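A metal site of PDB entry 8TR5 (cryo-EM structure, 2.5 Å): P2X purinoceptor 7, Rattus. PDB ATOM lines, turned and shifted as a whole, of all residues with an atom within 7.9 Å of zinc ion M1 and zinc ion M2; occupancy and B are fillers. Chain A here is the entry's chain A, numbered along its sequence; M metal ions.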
ATOM      1  N   VAL A 404     -31.315  23.668  20.770  1.00  0.00           N
ATOM      2  CA  VAL A 404     -31.604  23.584  19.353  1.00  0.00           C
ATOM      3  C   VAL A 404     -33.086  23.355  19.097  1.00  0.00           C
ATOM      4  O   VAL A 404     -33.555  23.537  17.966  1.00  0.00           O
ATOM      5  CB  VAL A 404     -30.743  22.495  18.704  1.00  0.00           C
ATOM      6  CG1 VAL A 404     -31.130  21.143  19.224  1.00  0.00           C
ATOM      7  CG2 VAL A 404     -30.891  22.538  17.209  1.00  0.00           C
ATOM      8  N   GLN A 422     -29.044  22.534  33.197  1.00  0.00           N
ATOM      9  CA  GLN A 422     -30.141  22.248  32.297  1.00  0.00           C
ATOM     10  C   GLN A 422     -31.475  22.530  32.970  1.00  0.00           C
ATOM     11  O   GLN A 422     -32.386  23.093  32.347  1.00  0.00           O
ATOM     12  CB  GLN A 422     -30.062  20.791  31.852  1.00  0.00           C
ATOM     13  CG  GLN A 422     -31.160  20.330  30.936  1.00  0.00           C
ATOM     14  CD  GLN A 422     -30.865  20.605  29.489  1.00  0.00           C
ATOM     15  OE1 GLN A 422     -29.865  21.217  29.153  1.00  0.00           O
ATOM     16  NE2 GLN A 422     -31.737  20.132  28.624  1.00  0.00           N
ATOM     17  N   SER A 473     -27.446   6.798  29.998  1.00  0.00           N
ATOM     18  CA  SER A 473     -27.142   8.196  29.744  1.00  0.00           C
ATOM     19  C   SER A 473     -27.624   9.063  30.907  1.00  0.00           C
ATOM     20  O   SER A 473     -28.503   8.666  31.667  1.00  0.00           O
ATOM     21  CB  SER A 473     -27.795   8.650  28.449  1.00  0.00           C
ATOM     22  OG  SER A 473     -28.015  10.047  28.451  1.00  0.00           O
ATOM     23  N   PRO A 474     -27.046  10.255  31.066  1.00  0.00           N
ATOM     24  CA  PRO A 474     -27.453  11.124  32.164  1.00  0.00           C
ATOM     25  C   PRO A 474     -28.926  11.479  32.108  1.00  0.00           C
ATOM     26  O   PRO A 474     -29.520  11.588  31.036  1.00  0.00           O
ATOM     27  CB  PRO A 474     -26.579  12.361  31.988  1.00  0.00           C
ATOM     28  CG  PRO A 474     -25.406  11.886  31.245  1.00  0.00           C
ATOM     29  CD  PRO A 474     -25.881  10.795  30.353  1.00  0.00           C
ATOM     30  N   TRP A 476     -30.408  14.291  32.941  1.00  0.00           N
ATOM     31  CA  TRP A 476     -30.611  15.607  32.356  1.00  0.00           C
ATOM     32  C   TRP A 476     -30.375  15.631  30.855  1.00  0.00           C
ATOM     33  O   TRP A 476     -30.679  16.647  30.217  1.00  0.00           O
ATOM     34  CB  TRP A 476     -29.710  16.636  33.030  1.00  0.00           C
ATOM     35  CG  TRP A 476     -28.295  16.201  33.201  1.00  0.00           C
ATOM     36  CD1 TRP A 476     -27.747  15.656  34.316  1.00  0.00           C
ATOM     37  CD2 TRP A 476     -27.252  16.260  32.237  1.00  0.00           C
ATOM     38  NE1 TRP A 476     -26.427  15.364  34.110  1.00  0.00           N
ATOM     39  CE2 TRP A 476     -26.099  15.729  32.834  1.00  0.00           C
ATOM     40  CE3 TRP A 476     -27.185  16.712  30.915  1.00  0.00           C
ATOM     41  CZ2 TRP A 476     -24.890  15.645  32.166  1.00  0.00           C
ATOM     42  CZ3 TRP A 476     -25.990  16.615  30.260  1.00  0.00           C
ATOM     43  CH2 TRP A 476     -24.857  16.089  30.879  1.00  0.00           C
ATOM     44  N   CYS A 477     -29.847  14.555  30.276  1.00  0.00           N
ATOM     45  CA  CYS A 477     -29.591  14.525  28.845  1.00  0.00           C
ATOM     46  C   CYS A 477     -30.835  14.068  28.104  1.00  0.00           C
ATOM     47  O   CYS A 477     -31.414  13.025  28.420  1.00  0.00           O
ATOM     48  CB  CYS A 477     -28.425  13.595  28.520  1.00  0.00           C
ATOM     49  SG  CYS A 477     -28.219  13.313  26.764  1.00  0.00           S
ATOM     50  N   GLN A 478     -31.227  14.841  27.097  1.00  0.00           N
ATOM     51  CA  GLN A 478     -32.365  14.529  26.255  1.00  0.00           C
ATOM     52  C   GLN A 478     -31.941  14.214  24.818  1.00  0.00           C
ATOM     53  O   GLN A 478     -32.745  14.317  23.893  1.00  0.00           O
ATOM     54  CB  GLN A 478     -33.366  15.677  26.267  1.00  0.00           C
ATOM     55  CG  GLN A 478     -33.547  16.337  27.617  1.00  0.00           C
ATOM     56  CD  GLN A 478     -34.497  15.592  28.518  1.00  0.00           C
ATOM     57  OE1 GLN A 478     -34.663  14.373  28.395  1.00  0.00           O
ATOM     58  NE2 GLN A 478     -35.104  16.303  29.443  1.00  0.00           N
ATOM     59  N   CYS A 479     -30.678  13.847  24.628  1.00  0.00           N
ATOM     60  CA  CYS A 479     -30.147  13.541  23.310  1.00  0.00           C
ATOM     61  C   CYS A 479     -29.363  12.245  23.231  1.00  0.00           C
ATOM     62  O   CYS A 479     -29.177  11.726  22.132  1.00  0.00           O
ATOM     63  CB  CYS A 479     -29.247  14.698  22.822  1.00  0.00           C
ATOM     64  SG  CYS A 479     -27.538  14.682  23.421  1.00  0.00           S
ATOM     65  N   GLY A 480     -28.906  11.699  24.367  1.00  0.00           N
ATOM     66  CA  GLY A 480     -28.220  10.436  24.385  1.00  0.00           C
ATOM     67  C   GLY A 480     -26.719  10.508  24.204  1.00  0.00           C
ATOM     68  O   GLY A 480     -26.034   9.516  24.479  1.00  0.00           O
ATOM     69  N   ASN A 481     -26.187  11.641  23.772  1.00  0.00           N
ATOM     70  CA  ASN A 481     -24.773  11.787  23.502  1.00  0.00           C
ATOM     71  C   ASN A 481     -24.012  12.503  24.605  1.00  0.00           C
ATOM     72  O   ASN A 481     -22.777  12.553  24.554  1.00  0.00           O
ATOM     73  CB  ASN A 481     -24.557  12.536  22.182  1.00  0.00           C
ATOM     74  CG  ASN A 481     -24.810  11.667  20.972  1.00  0.00           C
ATOM     75  OD1 ASN A 481     -25.857  11.771  20.319  1.00  0.00           O
ATOM     76  ND2 ASN A 481     -23.861  10.795  20.659  1.00  0.00           N
ATOM     77  N   CYS A 482     -24.702  13.034  25.600  1.00  0.00           N
ATOM     78  CA  CYS A 482     -24.037  13.755  26.676  1.00  0.00           C
ATOM     79  C   CYS A 482     -23.437  12.781  27.677  1.00  0.00           C
ATOM     80  O   CYS A 482     -23.893  11.644  27.832  1.00  0.00           O
ATOM     81  CB  CYS A 482     -25.003  14.702  27.366  1.00  0.00           C
ATOM     82  SG  CYS A 482     -25.559  16.074  26.357  1.00  0.00           S
ATOM     83  N   LEU A 483     -22.412  13.245  28.378  1.00  0.00           N
ATOM     84  CA  LEU A 483     -21.642  12.441  29.303  1.00  0.00           C
ATOM     85  C   LEU A 483     -21.489  13.181  30.629  1.00  0.00           C
ATOM     86  O   LEU A 483     -21.615  14.410  30.678  1.00  0.00           O
ATOM     87  CB  LEU A 483     -20.251  12.125  28.740  1.00  0.00           C
ATOM     88  CG  LEU A 483     -20.229  11.392  27.399  1.00  0.00           C
ATOM     89  CD1 LEU A 483     -18.845  11.311  26.778  1.00  0.00           C
ATOM     90  CD2 LEU A 483     -20.998  10.072  27.339  1.00  0.00           C
ATOM     91  N   LEU A 497     -25.326  20.106  31.051  1.00  0.00           N
ATOM     92  CA  LEU A 497     -26.206  20.776  30.117  1.00  0.00           C
ATOM     93  C   LEU A 497     -26.297  19.976  28.832  1.00  0.00           C
ATOM     94  O   LEU A 497     -25.289  19.455  28.350  1.00  0.00           O
ATOM     95  CB  LEU A 497     -25.713  22.193  29.836  1.00  0.00           C
ATOM     96  CG  LEU A 497     -26.491  23.061  28.866  1.00  0.00           C
ATOM     97  CD1 LEU A 497     -27.681  23.674  29.526  1.00  0.00           C
ATOM     98  CD2 LEU A 497     -25.582  24.122  28.360  1.00  0.00           C
ATOM     99  N   CYS A 498     -27.500  19.899  28.276  1.00  0.00           N
ATOM    100  CA  CYS A 498     -27.752  19.164  27.052  1.00  0.00           C
ATOM    101  C   CYS A 498     -27.966  20.115  25.887  1.00  0.00           C
ATOM    102  O   CYS A 498     -28.206  21.309  26.054  1.00  0.00           O
ATOM    103  CB  CYS A 498     -28.975  18.262  27.200  1.00  0.00           C
ATOM    104  SG  CYS A 498     -29.155  17.009  25.931  1.00  0.00           S
ATOM    105  N   CYS A 499     -27.878  19.559  24.676  1.00  0.00           N
ATOM    106  CA  CYS A 499     -28.083  20.344  23.467  1.00  0.00           C
ATOM    107  C   CYS A 499     -29.536  20.750  23.287  1.00  0.00           C
ATOM    108  O   CYS A 499     -29.802  21.781  22.660  1.00  0.00           O
ATOM    109  CB  CYS A 499     -27.615  19.561  22.247  1.00  0.00           C
ATOM    110  SG  CYS A 499     -28.435  18.002  21.989  1.00  0.00           S
ATOM    111  N   ARG A 500     -30.473  19.973  23.819  1.00  0.00           N
ATOM    112  CA  ARG A 500     -31.882  20.250  23.646  1.00  0.00           C
ATOM    113  C   ARG A 500     -32.611  20.060  24.963  1.00  0.00           C
ATOM    114  O   ARG A 500     -32.174  19.301  25.840  1.00  0.00           O
ATOM    115  CB  ARG A 500     -32.511  19.364  22.573  1.00  0.00           C
ATOM    116  CG  ARG A 500     -32.158  17.903  22.682  1.00  0.00           C
ATOM    117  CD  ARG A 500     -32.672  17.172  21.478  1.00  0.00           C
ATOM    118  NE  ARG A 500     -33.999  17.637  21.113  1.00  0.00           N
ATOM    119  CZ  ARG A 500     -34.388  17.988  19.890  1.00  0.00           C
ATOM    120  NH1 ARG A 500     -33.553  17.922  18.867  1.00  0.00           N
ATOM    121  NH2 ARG A 500     -35.626  18.408  19.700  1.00  0.00           N
ATOM    122  N   GLY A 504     -34.918  14.286  21.498  1.00  0.00           N
ATOM    123  CA  GLY A 504     -34.754  14.438  20.072  1.00  0.00           C
ATOM    124  C   GLY A 504     -33.340  14.074  19.661  1.00  0.00           C
ATOM    125  O   GLY A 504     -32.601  13.438  20.418  1.00  0.00           O
ATOM    126  N   GLN A 505     -32.987  14.494  18.461  1.00  0.00           N
ATOM    127  CA  GLN A 505     -31.661  14.200  17.931  1.00  0.00           C
ATOM    128  C   GLN A 505     -30.655  15.235  18.397  1.00  0.00           C
ATOM    129  O   GLN A 505     -30.973  16.422  18.545  1.00  0.00           O
ATOM    130  CB  GLN A 505     -31.698  14.147  16.400  1.00  0.00           C
ATOM    131  CG  GLN A 505     -32.416  15.310  15.750  1.00  0.00           C
ATOM    132  CD  GLN A 505     -32.097  15.436  14.277  1.00  0.00           C
ATOM    133  OE1 GLN A 505     -31.044  14.987  13.814  1.00  0.00           O
ATOM    134  NE2 GLN A 505     -32.999  16.044  13.535  1.00  0.00           N
ATOM    135  N   CYS A 506     -29.432  14.781  18.633  1.00  0.00           N
ATOM    136  CA  CYS A 506     -28.372  15.675  19.075  1.00  0.00           C
ATOM    137  C   CYS A 506     -27.952  16.606  17.947  1.00  0.00           C
ATOM    138  O   CYS A 506     -27.975  16.251  16.762  1.00  0.00           O
ATOM    139  CB  CYS A 506     -27.175  14.868  19.567  1.00  0.00           C
ATOM    140  SG  CYS A 506     -25.830  15.845  20.217  1.00  0.00           S
ATOM    141  N   ILE A 507     -27.560  17.818  18.334  1.00  0.00           N
ATOM    142  CA  ILE A 507     -27.073  18.803  17.373  1.00  0.00           C
ATOM    143  C   ILE A 507     -25.799  18.302  16.708  1.00  0.00           C
ATOM    144  O   ILE A 507     -25.465  18.736  15.590  1.00  0.00           O
ATOM    145  CB  ILE A 507     -26.867  20.150  18.073  1.00  0.00           C
ATOM    146  CG1 ILE A 507     -26.681  21.255  17.054  1.00  0.00           C
ATOM    147  CG2 ILE A 507     -25.673  20.082  18.970  1.00  0.00           C
ATOM    148  CD1 ILE A 507     -26.635  22.607  17.666  1.00  0.00           C
ATOM    149  N   THR A 508     -25.082  17.406  17.365  1.00  0.00           N
ATOM    150  CA  THR A 508     -23.877  16.833  16.780  1.00  0.00           C
ATOM    151  C   THR A 508     -24.166  16.043  15.514  1.00  0.00           C
ATOM    152  O   THR A 508     -23.264  15.823  14.708  1.00  0.00           O
ATOM    153  CB  THR A 508     -23.185  15.930  17.786  1.00  0.00           C
ATOM    154  OG1 THR A 508     -24.088  14.918  18.241  1.00  0.00           O
ATOM    155  CG2 THR A 508     -22.716  16.730  18.962  1.00  0.00           C
ATOM    156  N   THR A 509     -25.412  15.596  15.325  1.00  0.00           N
ATOM    157  CA  THR A 509     -25.767  14.868  14.124  1.00  0.00           C
ATOM    158  C   THR A 509     -25.846  15.777  12.908  1.00  0.00           C
ATOM    159  O   THR A 509     -25.766  15.291  11.774  1.00  0.00           O
ATOM    160  CB  THR A 509     -27.099  14.149  14.324  1.00  0.00           C
ATOM    161  OG1 THR A 509     -28.142  15.106  14.476  1.00  0.00           O
ATOM    162  CG2 THR A 509     -27.028  13.272  15.562  1.00  0.00           C
ATOM    163  N   PRO A 570     -22.886  22.438  25.498  1.00  0.00           N
ATOM    164  CA  PRO A 570     -23.458  21.188  25.996  1.00  0.00           C
ATOM    165  C   PRO A 570     -22.406  20.122  26.193  1.00  0.00           C
ATOM    166  O   PRO A 570     -21.327  20.159  25.587  1.00  0.00           O
ATOM    167  CB  PRO A 570     -24.453  20.802  24.898  1.00  0.00           C
ATOM    168  CG  PRO A 570     -24.744  22.031  24.205  1.00  0.00           C
ATOM    169  CD  PRO A 570     -23.516  22.840  24.234  1.00  0.00           C
ATOM    170  N   SER A 571     -22.711  19.166  27.054  1.00  0.00           N
ATOM    171  CA  SER A 571     -21.779  18.076  27.296  1.00  0.00           C
ATOM    172  C   SER A 571     -21.541  17.257  26.039  1.00  0.00           C
ATOM    173  O   SER A 571     -20.421  16.826  25.779  1.00  0.00           O
ATOM    174  CB  SER A 571     -22.304  17.182  28.418  1.00  0.00           C
ATOM    175  OG  SER A 571     -21.250  16.491  29.068  1.00  0.00           O
ATOM    176  N   CYS A 572     -22.592  17.051  25.240  1.00  0.00           N
ATOM    177  CA  CYS A 572     -22.442  16.270  24.021  1.00  0.00           C
ATOM    178  C   CYS A 572     -21.469  16.926  23.060  1.00  0.00           C
ATOM    179  O   CYS A 572     -20.508  16.288  22.604  1.00  0.00           O
ATOM    180  CB  CYS A 572     -23.808  16.081  23.366  1.00  0.00           C
ATOM    181  SG  CYS A 572     -24.832  17.560  23.299  1.00  0.00           S
ATOM    182  N   CYS A 573     -21.674  18.200  22.754  1.00  0.00           N
ATOM    183  CA  CYS A 573     -20.801  18.902  21.834  1.00  0.00           C
ATOM    184  C   CYS A 573     -19.395  19.055  22.410  1.00  0.00           C
ATOM    185  O   CYS A 573     -18.401  18.870  21.699  1.00  0.00           O
ATOM    186  CB  CYS A 573     -21.411  20.262  21.499  1.00  0.00           C
ATOM    187  SG  CYS A 573     -23.147  20.164  21.078  1.00  0.00           S
HETATM  188 ZN    ZN M   1     -27.624  15.275  25.659  1.00  0.00          ZN
HETATM  189 ZN    ZN M   2     -26.654  16.531  22.285  1.00  0.00          ZN
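Residues that only touch zinc ion M1: Gln 478 (3.9 Å). Five residues have an atom within 4 Å of zinc ion M1: Cys 477, Gln 478, Cys 479, Cys 482 and Cys 498. The nearest printed residue that does not touch zinc ion M1 is Gly 480 (4.01 Å).
Zinc ion M1 is bound by SG of Cys 479 (2.3 Å), SG of Cys 482 (2.3 Å), SG of Cys 477 (2.3 Å) and SG of Cys 498 (2.3 Å).
SG of Cys 479 sits close to N of Asn 481 (3.3 Å). The side-chain sulfur of Cys 482 sits close to the backbone NH of Cys 572, 3.3 Å away. The side-chain sulfur of Cys 477 sits close to the backbone NH of Gly 480. The side-chain sulfur (SG) of Cys 477 lies close to the side-chain hydroxyl (OG) of Ser 473, at 3.7 Å. N of Ile 507 lies close to SG of Cys 499 (3.8 Å). The side-chain sulfur of Cys 506 lies close to the side-chain hydroxyl of Thr 508. The side-chain hydroxyl (OG1) of Thr 509 lies within hydrogen-bond range of the backbone carbonyl oxygen (O) of Cys 506. The backbone NH (N) of Gly 504 sits at hydrogen-bond distance from the backbone carbonyl oxygen (O) of Gln 478 (3.2 Å).
Within 4 Å of zinc ion M2: Cys 479, Cys 499, Cys 506 and Cys 572.
Zinc ion M2 is bound by the side-chain sulfur (SG) of Cys 572 (2.3 Å), the side-chain sulfur (SG) of Cys 499 (2.3 Å), the side-chain sulfur (SG) of Cys 506 (2.3 Å) and the side-chain sulfur (SG) of Cys 479 (2.3 Å).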
